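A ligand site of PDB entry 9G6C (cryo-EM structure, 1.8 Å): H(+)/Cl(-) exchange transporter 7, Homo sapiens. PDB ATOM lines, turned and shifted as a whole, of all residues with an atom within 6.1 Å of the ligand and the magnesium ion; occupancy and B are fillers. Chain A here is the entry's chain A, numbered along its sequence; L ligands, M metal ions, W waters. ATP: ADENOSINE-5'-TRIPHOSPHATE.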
ATOM      1  N   LEU A  92     -31.247   6.183   4.953  1.00  0.00           N
ATOM      2  CA  LEU A  92     -30.429   6.544   6.106  1.00  0.00           C
ATOM      3  C   LEU A  92     -30.309   8.054   6.300  1.00  0.00           C
ATOM      4  O   LEU A  92     -29.689   8.487   7.274  1.00  0.00           O
ATOM      5  CB  LEU A  92     -29.027   5.936   5.985  1.00  0.00           C
ATOM      6  CG  LEU A  92     -28.771   4.450   6.288  1.00  0.00           C
ATOM      7  CD1 LEU A  92     -29.859   3.513   5.764  1.00  0.00           C
ATOM      8  CD2 LEU A  92     -27.415   4.028   5.767  1.00  0.00           C
ATOM      9  N   TYR A  94     -32.998  10.055   6.655  1.00  0.00           N
ATOM     10  CA  TYR A  94     -34.144  10.517   7.416  1.00  0.00           C
ATOM     11  C   TYR A  94     -33.882  10.362   8.908  1.00  0.00           C
ATOM     12  O   TYR A  94     -33.471   9.300   9.367  1.00  0.00           O
ATOM     13  CB  TYR A  94     -35.400   9.757   7.016  1.00  0.00           C
ATOM     14  CG  TYR A  94     -35.728   9.812   5.541  1.00  0.00           C
ATOM     15  CD1 TYR A  94     -36.250  10.960   4.977  1.00  0.00           C
ATOM     16  CD2 TYR A  94     -35.511   8.712   4.712  1.00  0.00           C
ATOM     17  CE1 TYR A  94     -36.548  11.024   3.627  1.00  0.00           C
ATOM     18  CE2 TYR A  94     -35.805   8.764   3.368  1.00  0.00           C
ATOM     19  CZ  TYR A  94     -36.326   9.916   2.826  1.00  0.00           C
ATOM     20  OH  TYR A  94     -36.618   9.981   1.488  1.00  0.00           O
ATOM     21  N   GLU A  95     -34.125  11.436   9.657  1.00  0.00           N
ATOM     22  CA  GLU A  95     -33.924  11.445  11.100  1.00  0.00           C
ATOM     23  C   GLU A  95     -35.262  11.514  11.816  1.00  0.00           C
ATOM     24  O   GLU A  95     -36.173  12.233  11.389  1.00  0.00           O
ATOM     25  CB  GLU A  95     -33.044  12.629  11.528  1.00  0.00           C
ATOM     26  CG  GLU A  95     -31.689  12.704  10.826  1.00  0.00           C
ATOM     27  CD  GLU A  95     -30.672  11.703  11.348  1.00  0.00           C
ATOM     28  OE1 GLU A  95     -31.070  10.726  12.007  1.00  0.00           O
ATOM     29  OE2 GLU A  95     -29.472  11.900  11.089  1.00  0.00           O
ATOM     30  N   SER A  96     -35.379  10.777  12.912  1.00  0.00           N
ATOM     31  CA  SER A  96     -36.617  10.743  13.677  1.00  0.00           C
ATOM     32  C   SER A  96     -36.752  11.972  14.564  1.00  0.00           C
ATOM     33  O   SER A  96     -35.757  12.613  14.924  1.00  0.00           O
ATOM     34  CB  SER A  96     -36.693   9.475  14.520  1.00  0.00           C
ATOM     35  OG  SER A  96     -36.453   8.327  13.743  1.00  0.00           O
ATOM     36  N   LEU A  97     -37.987  12.303  14.917  1.00  0.00           N
ATOM     37  CA  LEU A  97     -38.248  13.379  15.845  1.00  0.00           C
ATOM     38  C   LEU A  97     -37.834  12.983  17.257  1.00  0.00           C
ATOM     39  O   LEU A  97     -37.828  11.800  17.621  1.00  0.00           O
ATOM     40  CB  LEU A  97     -39.728  13.768  15.832  1.00  0.00           C
ATOM     41  CG  LEU A  97     -40.270  14.496  14.608  1.00  0.00           C
ATOM     42  CD1 LEU A  97     -41.775  14.311  14.510  1.00  0.00           C
ATOM     43  CD2 LEU A  97     -39.931  15.980  14.703  1.00  0.00           C
ATOM     44  N   MET A 631     -32.554  -5.806  17.837  1.00  0.00           N
ATOM     45  CA  MET A 631     -31.726  -4.729  18.337  1.00  0.00           C
ATOM     46  C   MET A 631     -30.402  -4.652  17.564  1.00  0.00           C
ATOM     47  O   MET A 631     -29.958  -5.605  16.923  1.00  0.00           O
ATOM     48  CB  MET A 631     -31.450  -4.915  19.825  1.00  0.00           C
ATOM     49  CG  MET A 631     -30.352  -5.916  20.124  1.00  0.00           C
ATOM     50  SD  MET A 631     -30.283  -6.388  21.862  1.00  0.00           S
ATOM     51  CE  MET A 631     -29.182  -7.794  21.793  1.00  0.00           C
ATOM     52  N   SER A 632     -29.787  -3.469  17.620  1.00  0.00           N
ATOM     53  CA  SER A 632     -28.484  -3.239  17.016  1.00  0.00           C
ATOM     54  C   SER A 632     -27.407  -3.344  18.079  1.00  0.00           C
ATOM     55  O   SER A 632     -27.495  -2.699  19.133  1.00  0.00           O
ATOM     56  CB  SER A 632     -28.437  -1.860  16.346  1.00  0.00           C
ATOM     57  OG  SER A 632     -28.490  -0.822  17.314  1.00  0.00           O
ATOM     58  N   THR A 633     -26.386  -4.157  17.802  1.00  0.00           N
ATOM     59  CA  THR A 633     -25.299  -4.411  18.737  1.00  0.00           C
ATOM     60  C   THR A 633     -24.020  -4.559  17.938  1.00  0.00           C
ATOM     61  O   THR A 633     -24.055  -5.069  16.813  1.00  0.00           O
ATOM     62  CB  THR A 633     -25.566  -5.666  19.579  1.00  0.00           C
ATOM     63  OG1 THR A 633     -24.455  -5.911  20.460  1.00  0.00           O
ATOM     64  CG2 THR A 633     -25.784  -6.887  18.688  1.00  0.00           C
ATOM     65  N   PRO A 634     -22.867  -4.108  18.478  1.00  0.00           N
ATOM     66  CA  PRO A 634     -22.649  -3.453  19.776  1.00  0.00           C
ATOM     67  C   PRO A 634     -23.141  -2.010  19.804  1.00  0.00           C
ATOM     68  O   PRO A 634     -23.381  -1.399  18.761  1.00  0.00           O
ATOM     69  CB  PRO A 634     -21.128  -3.542  19.941  1.00  0.00           C
ATOM     70  CG  PRO A 634     -20.612  -3.440  18.537  1.00  0.00           C
ATOM     71  CD  PRO A 634     -21.612  -4.212  17.709  1.00  0.00           C
ATOM     72  N   VAL A 635     -23.302  -1.433  20.997  1.00  0.00           N
ATOM     73  CA  VAL A 635     -23.839  -0.098  21.170  1.00  0.00           C
ATOM     74  C   VAL A 635     -22.711   0.853  21.529  1.00  0.00           C
ATOM     75  O   VAL A 635     -21.877   0.550  22.396  1.00  0.00           O
ATOM     76  CB  VAL A 635     -24.923  -0.078  22.262  1.00  0.00           C
ATOM     77  CG1 VAL A 635     -25.513   1.315  22.400  1.00  0.00           C
ATOM     78  CG2 VAL A 635     -26.009  -1.070  21.926  1.00  0.00           C
ATOM     79  N   THR A 636     -22.672   2.002  20.851  1.00  0.00           N
ATOM     80  CA  THR A 636     -21.728   3.061  21.184  1.00  0.00           C
ATOM     81  C   THR A 636     -22.287   3.835  22.378  1.00  0.00           C
ATOM     82  O   THR A 636     -23.278   4.568  22.249  1.00  0.00           O
ATOM     83  CB  THR A 636     -21.513   3.980  19.991  1.00  0.00           C
ATOM     84  OG1 THR A 636     -21.100   3.206  18.855  1.00  0.00           O
ATOM     85  CG2 THR A 636     -20.441   5.021  20.301  1.00  0.00           C
ATOM     86  N   CYS A 637     -21.663   3.664  23.534  1.00  0.00           N
ATOM     87  CA  CYS A 637     -22.115   4.282  24.768  1.00  0.00           C
ATOM     88  C   CYS A 637     -21.102   5.312  25.257  1.00  0.00           C
ATOM     89  O   CYS A 637     -19.964   5.371  24.789  1.00  0.00           O
ATOM     90  CB  CYS A 637     -22.355   3.215  25.853  1.00  0.00           C
ATOM     91  SG  CYS A 637     -23.579   1.962  25.412  1.00  0.00           S
ATOM     92  N   SER A 656     -20.757   6.121  10.799  1.00  0.00           N
ATOM     93  CA  SER A 656     -22.140   6.124  11.247  1.00  0.00           C
ATOM     94  C   SER A 656     -22.498   7.520  11.730  1.00  0.00           C
ATOM     95  O   SER A 656     -21.627   8.357  11.980  1.00  0.00           O
ATOM     96  CB  SER A 656     -22.372   5.094  12.365  1.00  0.00           C
ATOM     97  OG  SER A 656     -21.656   5.446  13.540  1.00  0.00           O
ATOM     98  N   ASN A 657     -23.805   7.762  11.862  1.00  0.00           N
ATOM     99  CA  ASN A 657     -24.334   9.054  12.288  1.00  0.00           C
ATOM    100  C   ASN A 657     -25.380   8.865  13.370  1.00  0.00           C
ATOM    101  O   ASN A 657     -26.489   9.387  13.308  1.00  0.00           O
ATOM    102  CB  ASN A 657     -24.904   9.816  11.096  1.00  0.00           C
ATOM    103  CG  ASN A 657     -25.210  11.267  11.425  1.00  0.00           C
ATOM    104  OD1 ASN A 657     -24.426  11.932  12.120  1.00  0.00           O
ATOM    105  ND2 ASN A 657     -26.331  11.772  10.926  1.00  0.00           N
ATOM    106  N   HIS A 658     -25.028   8.083  14.392  1.00  0.00           N
ATOM    107  CA  HIS A 658     -25.936   7.859  15.509  1.00  0.00           C
ATOM    108  C   HIS A 658     -26.239   9.167  16.215  1.00  0.00           C
ATOM    109  O   HIS A 658     -25.365  10.021  16.388  1.00  0.00           O
ATOM    110  CB  HIS A 658     -25.326   6.857  16.497  1.00  0.00           C
ATOM    111  CG  HIS A 658     -24.847   5.596  15.864  1.00  0.00           C
ATOM    112  ND1 HIS A 658     -25.562   4.935  14.882  1.00  0.00           N
ATOM    113  CD2 HIS A 658     -23.722   4.861  16.059  1.00  0.00           C
ATOM    114  CE1 HIS A 658     -24.901   3.849  14.511  1.00  0.00           C
ATOM    115  NE2 HIS A 658     -23.782   3.784  15.214  1.00  0.00           N
ATOM    116  N   ASN A 659     -27.499   9.328  16.632  1.00  0.00           N
ATOM    117  CA  ASN A 659     -27.938  10.543  17.312  1.00  0.00           C
ATOM    118  C   ASN A 659     -28.330  10.299  18.758  1.00  0.00           C
ATOM    119  O   ASN A 659     -28.654  11.269  19.462  1.00  0.00           O
ATOM    120  CB  ASN A 659     -29.118  11.165  16.553  1.00  0.00           C
ATOM    121  CG  ASN A 659     -28.694  11.844  15.269  1.00  0.00           C
ATOM    122  OD1 ASN A 659     -28.103  12.915  15.283  1.00  0.00           O
ATOM    123  ND2 ASN A 659     -28.994  11.201  14.141  1.00  0.00           N
ATOM    124  N   GLY A 660     -28.298   9.068  19.233  1.00  0.00           N
ATOM    125  CA  GLY A 660     -28.570   8.769  20.622  1.00  0.00           C
ATOM    126  C   GLY A 660     -27.544   7.805  21.179  1.00  0.00           C
ATOM    127  O   GLY A 660     -27.168   6.839  20.516  1.00  0.00           O
ATOM    128  N   PHE A 661     -27.099   8.086  22.404  1.00  0.00           N
ATOM    129  CA  PHE A 661     -26.028   7.321  23.031  1.00  0.00           C
ATOM    130  C   PHE A 661     -26.426   7.008  24.458  1.00  0.00           C
ATOM    131  O   PHE A 661     -26.618   7.938  25.266  1.00  0.00           O
ATOM    132  CB  PHE A 661     -24.710   8.103  22.982  1.00  0.00           C
ATOM    133  CG  PHE A 661     -24.291   8.495  21.599  1.00  0.00           C
ATOM    134  CD1 PHE A 661     -23.585   7.618  20.797  1.00  0.00           C
ATOM    135  CD2 PHE A 661     -24.604   9.749  21.095  1.00  0.00           C
ATOM    136  CE1 PHE A 661     -23.201   7.982  19.516  1.00  0.00           C
ATOM    137  CE2 PHE A 661     -24.224  10.117  19.823  1.00  0.00           C
ATOM    138  CZ  PHE A 661     -23.518   9.232  19.036  1.00  0.00           C
ATOM    139  N   PRO A 662     -26.584   5.730  24.820  1.00  0.00           N
ATOM    140  CA  PRO A 662     -26.829   5.396  26.223  1.00  0.00           C
ATOM    141  C   PRO A 662     -25.664   5.820  27.104  1.00  0.00           C
ATOM    142  O   PRO A 662     -24.499   5.729  26.711  1.00  0.00           O
ATOM    143  CB  PRO A 662     -26.993   3.864  26.195  1.00  0.00           C
ATOM    144  CG  PRO A 662     -27.323   3.537  24.780  1.00  0.00           C
ATOM    145  CD  PRO A 662     -26.589   4.547  23.950  1.00  0.00           C
ATOM    146  N   ARG A 767     -37.531   7.470  19.923  1.00  0.00           N
ATOM    147  CA  ARG A 767     -36.466   7.459  18.935  1.00  0.00           C
ATOM    148  C   ARG A 767     -35.396   6.428  19.236  1.00  0.00           C
ATOM    149  O   ARG A 767     -34.865   5.808  18.312  1.00  0.00           O
ATOM    150  CB  ARG A 767     -35.819   8.851  18.856  1.00  0.00           C
ATOM    151  CG  ARG A 767     -34.763   8.976  17.771  1.00  0.00           C
ATOM    152  CD  ARG A 767     -34.212  10.385  17.680  1.00  0.00           C
ATOM    153  NE  ARG A 767     -33.441  10.595  16.469  1.00  0.00           N
ATOM    154  CZ  ARG A 767     -32.720  11.687  16.212  1.00  0.00           C
ATOM    155  NH1 ARG A 767     -32.642  12.679  17.089  1.00  0.00           N
ATOM    156  NH2 ARG A 767     -32.063  11.777  15.066  1.00  0.00           N
ATOM    157  N   HIS A 768     -35.069   6.215  20.512  1.00  0.00           N
ATOM    158  CA  HIS A 768     -34.101   5.219  20.932  1.00  0.00           C
ATOM    159  C   HIS A 768     -34.691   4.402  22.060  1.00  0.00           C
ATOM    160  O   HIS A 768     -35.175   4.963  23.052  1.00  0.00           O
ATOM    161  CB  HIS A 768     -32.787   5.872  21.366  1.00  0.00           C
ATOM    162  CG  HIS A 768     -32.161   6.732  20.314  1.00  0.00           C
ATOM    163  ND1 HIS A 768     -32.317   8.104  20.285  1.00  0.00           N
ATOM    164  CD2 HIS A 768     -31.380   6.421  19.251  1.00  0.00           C
ATOM    165  CE1 HIS A 768     -31.661   8.602  19.252  1.00  0.00           C
ATOM    166  NE2 HIS A 768     -31.079   7.595  18.608  1.00  0.00           N
ATOM    167  N   LEU A 781     -29.631  -1.547  21.047  1.00  0.00           N
ATOM    168  CA  LEU A 781     -30.406  -0.329  20.863  1.00  0.00           C
ATOM    169  C   LEU A 781     -31.415  -0.542  19.744  1.00  0.00           C
ATOM    170  O   LEU A 781     -31.093  -1.148  18.720  1.00  0.00           O
ATOM    171  CB  LEU A 781     -29.511   0.872  20.535  1.00  0.00           C
ATOM    172  CG  LEU A 781     -30.069   2.245  20.880  1.00  0.00           C
ATOM    173  CD1 LEU A 781     -30.384   2.339  22.360  1.00  0.00           C
ATOM    174  CD2 LEU A 781     -29.105   3.342  20.462  1.00  0.00           C
ATOM    175  N   VAL A 782     -32.630  -0.035  19.937  1.00  0.00           N
ATOM    176  CA  VAL A 782     -33.716  -0.181  18.979  1.00  0.00           C
ATOM    177  C   VAL A 782     -34.131   1.208  18.516  1.00  0.00           C
ATOM    178  O   VAL A 782     -34.506   2.058  19.345  1.00  0.00           O
ATOM    179  CB  VAL A 782     -34.907  -0.942  19.568  1.00  0.00           C
ATOM    180  CG1 VAL A 782     -36.113  -0.828  18.647  1.00  0.00           C
ATOM    181  CG2 VAL A 782     -34.541  -2.402  19.787  1.00  0.00           C
ATOM    182  N   THR A 783     -34.063   1.440  17.214  1.00  0.00           N
ATOM    183  CA  THR A 783     -34.562   2.652  16.574  1.00  0.00           C
ATOM    184  C   THR A 783     -35.609   2.256  15.531  1.00  0.00           C
ATOM    185  O   THR A 783     -35.882   1.069  15.311  1.00  0.00           O
ATOM    186  CB  THR A 783     -33.435   3.462  15.939  1.00  0.00           C
ATOM    187  OG1 THR A 783     -32.925   2.761  14.798  1.00  0.00           O
ATOM    188  CG2 THR A 783     -32.315   3.692  16.943  1.00  0.00           C
ATOM    189  N   ARG A 784     -36.196   3.260  14.888  1.00  0.00           N
ATOM    190  CA  ARG A 784     -37.281   2.987  13.940  1.00  0.00           C
ATOM    191  C   ARG A 784     -36.799   2.174  12.743  1.00  0.00           C
ATOM    192  O   ARG A 784     -37.568   1.390  12.187  1.00  0.00           O
ATOM    193  CB  ARG A 784     -37.937   4.291  13.487  1.00  0.00           C
ATOM    194  CG  ARG A 784     -37.161   5.081  12.444  1.00  0.00           C
ATOM    195  CD  ARG A 784     -38.014   6.231  11.899  1.00  0.00           C
ATOM    196  NE  ARG A 784     -38.828   6.835  12.939  1.00  0.00           N
ATOM    197  CZ  ARG A 784     -40.155   6.851  12.940  1.00  0.00           C
ATOM    198  NH1 ARG A 784     -40.849   6.294  11.956  1.00  0.00           N
ATOM    199  NH2 ARG A 784     -40.797   7.432  13.942  1.00  0.00           N
ATOM    200  N   LYS A 785     -35.542   2.353  12.328  1.00  0.00           N
ATOM    201  CA  LYS A 785     -35.021   1.571  11.215  1.00  0.00           C
ATOM    202  C   LYS A 785     -34.927   0.092  11.567  1.00  0.00           C
ATOM    203  O   LYS A 785     -35.064  -0.774  10.694  1.00  0.00           O
ATOM    204  CB  LYS A 785     -33.652   2.103  10.785  1.00  0.00           C
ATOM    205  CG  LYS A 785     -33.732   3.222   9.759  1.00  0.00           C
ATOM    206  CD  LYS A 785     -32.352   3.628   9.260  1.00  0.00           C
ATOM    207  CE  LYS A 785     -32.034   5.067   9.633  1.00  0.00           C
ATOM    208  NZ  LYS A 785     -31.844   5.226  11.100  1.00  0.00           N
ATOM    209  N   ASP A 786     -34.684  -0.226  12.844  1.00  0.00           N
ATOM    210  CA  ASP A 786     -34.658  -1.629  13.264  1.00  0.00           C
ATOM    211  C   ASP A 786     -36.040  -2.259  13.198  1.00  0.00           C
ATOM    212  O   ASP A 786     -36.166  -3.445  12.873  1.00  0.00           O
ATOM    213  CB  ASP A 786     -34.086  -1.737  14.684  1.00  0.00           C
ATOM    214  CG  ASP A 786     -32.721  -1.097  14.808  1.00  0.00           C
ATOM    215  OD1 ASP A 786     -31.834  -1.402  13.993  1.00  0.00           O
ATOM    216  OD2 ASP A 786     -32.540  -0.269  15.727  1.00  0.00           O
HETATM  217  PG  ATP L   1     -32.989   7.911  13.786  1.00  0.00           P
HETATM  218  O1G ATP L   1     -33.520   9.288  14.001  1.00  0.00           O
HETATM  219  O2G ATP L   1     -34.025   6.807  13.982  1.00  0.00           O
HETATM  220  O3G ATP L   1     -32.307   7.722  12.434  1.00  0.00           O
HETATM  221  PB  ATP L   1     -30.269   7.621  14.988  1.00  0.00           P
HETATM  222  O1B ATP L   1     -29.700   8.784  14.281  1.00  0.00           O
HETATM  223  O2B ATP L   1     -29.934   7.505  16.469  1.00  0.00           O
HETATM  224  O3B ATP L   1     -31.848   7.586  14.853  1.00  0.00           O
HETATM  225  PA  ATP L   1     -29.077   5.800  12.990  1.00  0.00           P
HETATM  226  O1A ATP L   1     -27.621   5.956  13.151  1.00  0.00           O
HETATM  227  O2A ATP L   1     -29.676   6.584  11.823  1.00  0.00           O
HETATM  228  O3A ATP L   1     -29.856   6.244  14.298  1.00  0.00           O
HETATM  229  O5' ATP L   1     -29.490   4.286  12.832  1.00  0.00           O
HETATM  230  C5' ATP L   1     -28.676   3.360  12.082  1.00  0.00           C
HETATM  231  C4' ATP L   1     -28.504   2.083  12.876  1.00  0.00           C
HETATM  232  O4' ATP L   1     -27.601   2.316  13.979  1.00  0.00           O
HETATM  233  C3' ATP L   1     -29.781   1.499  13.469  1.00  0.00           C
HETATM  234  O3' ATP L   1     -29.804   0.078  13.345  1.00  0.00           O
HETATM  235  C2' ATP L   1     -29.718   1.939  14.938  1.00  0.00           C
HETATM  236  O2' ATP L   1     -30.386   1.025  15.788  1.00  0.00           O
HETATM  237  C1' ATP L   1     -28.209   1.910  15.189  1.00  0.00           C
HETATM  238  N9  ATP L   1     -27.773   2.814  16.257  1.00  0.00           N
HETATM  239  C8  ATP L   1     -28.310   4.029  16.574  1.00  0.00           C
HETATM  240  N7  ATP L   1     -27.710   4.632  17.582  1.00  0.00           N
HETATM  241  C5  ATP L   1     -26.710   3.745  17.944  1.00  0.00           C
HETATM  242  C6  ATP L   1     -25.718   3.777  18.936  1.00  0.00           C
HETATM  243  N6  ATP L   1     -25.560   4.792  19.800  1.00  0.00           N
HETATM  244  N1  ATP L   1     -24.879   2.725  19.028  1.00  0.00           N
HETATM  245  C2  ATP L   1     -25.025   1.707  18.182  1.00  0.00           C
HETATM  246  N3  ATP L   1     -25.911   1.560  17.199  1.00  0.00           N
HETATM  247  C4  ATP L   1     -26.736   2.621  17.133  1.00  0.00           C
HETATM  248 MG    MG M   1     -30.498   8.568  12.054  1.00  0.00          MG
HETATM  249  O   HOH W   1     -35.653   5.980  15.909  1.00  0.00           O
HETATM  250  O   HOH W   2     -25.120  -0.054  14.791  1.00  0.00           O
HETATM  251  O   HOH W   3     -28.663   9.208  11.436  1.00  0.00           O
HETATM  252  O   HOH W   4     -30.952   8.287  10.037  1.00  0.00           O
HETATM  253  O   HOH W   5     -34.711   6.987  10.735  1.00  0.00           O
HETATM  254  O   HOH W   6     -25.970   5.974  11.199  1.00  0.00           O
HETATM  255  O   HOH W   7     -27.182  -1.223  13.264  1.00  0.00           O
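Asn 659 touches the magnesium ion (ND2 to MG, 3.7 Å).
Lys 785 touches the magnesium ion (NZ to MG, 3.7 Å).
Within 4 Å of the magnesium ion: Glu 95, Asn 659 and Lys 785.
OE1 of Glu 95 lies close to NH2 of Arg 767 (3.4 Å).
OE2 of Glu 95 is in hydrogen-bond range of ND2 of Asn 657 (3.1 Å).
A ring nitrogen (NE2) of His 768 lies within hydrogen-bond range of the backbone NH (N) of Gly 660.
ND2 of Asn 659 sits at hydrogen-bond distance from O of Asn 657 (3.2 Å).
O of Ser 96 lies close to NE of Arg 767, 3.4 Å away.
The guanidinium group (NE) of Arg 784 is in hydrogen-bond range of the side-chain hydroxyl (OG) of Ser 96.
The backbone carbonyl oxygen (O) of Leu 781 is in hydrogen-bond range of the backbone NH (N) of Ser 632 (2.9 Å).
The side-chain sulfur (SG) of Cys 637 lies close to the backbone carbonyl oxygen (O) of Val 635, at 3.7 Å.
The backbone carbonyl oxygen (O) of Asn 657 lies close to an oxygen (O1B) of the ligand.
Tyr 94 touches the ligand (O to O3G, 3.6 Å).
O of Pro 634 touches C2 of the ligand, at 3.6 Å.
Val 635 touches the ligand.
Phe 661 touches the ligand (CD1 to N6, 3.6 Å).
Leu 781 touches the ligand.
CG of Arg 784 touches O2G of the ligand, at 3.9 Å.
Hydrophobic or aromatic side chains that line the ligand: Val 635, His 658, Phe 661, His 768 and Leu 781.
19 residues have an atom within 4 Å of the ligand: Tyr 94, Glu 95, Ser 96, Ser 632, Pro 634, Val 635, Thr 636, Asn 657, His 658, Asn 659, Gly 660, Phe 661, Arg 767, His 768, Leu 781, Thr 783, Arg 784, Lys 785 and Asp 786.
An oxygen (O2B) of the ligand is in hydrogen-bond range of a ring nitrogen (NE2) of His 768, at 2.4 Å.
An oxygen (O2') of the ligand sits at hydrogen-bond distance from the side-chain carboxylate (OD2) of Asp 786, 2.5 Å away.
The backbone NH of Asn 659 is in hydrogen-bond range of an oxygen (O2B) of the ligand, 3.0 Å away.
An oxygen (O1B) of the ligand lies close to the side-chain amide nitrogen (ND2) of Asn 659 (2.5 Å).
An oxygen (O1G) of the ligand lies within hydrogen-bond range of the backbone NH of Ser 96 (2.6 Å).
The side-chain hydroxyl of Ser 96 sits at hydrogen-bond distance from an oxygen (O2G) of the ligand, 2.9 Å away.
NZ of Lys 785 is in salt-bridge range of O2G of the ligand, at 3.9 Å.
A nitrogen (N6) of the ligand lies within hydrogen-bond range of the backbone carbonyl oxygen (O) of Gly 660 (2.7 Å).
The guanidinium group (NE) of Arg 767 lies within salt-bridge range of an oxygen (O1G) of the ligand.
ND1 of His 658 sits at hydrogen-bond distance from O1A of the ligand, at 2.9 Å.
N of Thr 636 sits at hydrogen-bond distance from N1 of the ligand, 3.0 Å away.
The backbone carbonyl oxygen (O) of Thr 636 sits at hydrogen-bond distance from a nitrogen (N6) of the ligand (3.4 Å).
O2' of the ligand sits at hydrogen-bond distance from OG of Ser 632, at 3.1 Å.
An oxygen (O2') of the ligand sits at hydrogen-bond distance from the side-chain hydroxyl (OG1) of Thr 783 (3.2 Å).
The magnesium ion is bound by an oxygen (O3G) of the ligand (2.0 Å), water W3 (2.0 Å), water W4 (2.1 Å), an oxygen (O2A) of the ligand (2.2 Å), the side-chain carboxylate (OE1) of Glu 95 (2.2 Å) and an oxygen (O1B) of the ligand (2.4 Å).
The magnesium ion has six donor atoms within binding distance.
Water W3 lies within hydrogen-bond range of OE2 of Glu 95, O of Asn 657 and ND2 of Asn 659.
Water W4 lies within hydrogen-bond range of the backbone carbonyl oxygen (O) of Tyr 94 (2.8 Å), the backbone carbonyl oxygen (O) of Leu 92 (3.0 Å) and the side-chain amino group (NZ) of Lys 785 (3.4 Å).
Water W6 lies within hydrogen-bond range of O1A of the ligand and N of Asn 657.
Water W1 lies within hydrogen-bond range of the backbone carbonyl oxygen (O) of Arg 767 (2.5 Å), an oxygen (O2G) of the ligand (2.7 Å), the backbone NH (N) of Arg 784 (3.0 Å) and the side-chain hydroxyl (OG) of Ser 96 (3.3 Å).
Water W5 lies within hydrogen-bond range of the backbone carbonyl oxygen of Tyr 94, an oxygen (O2G) of the ligand and the side-chain amino group of Lys 785.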
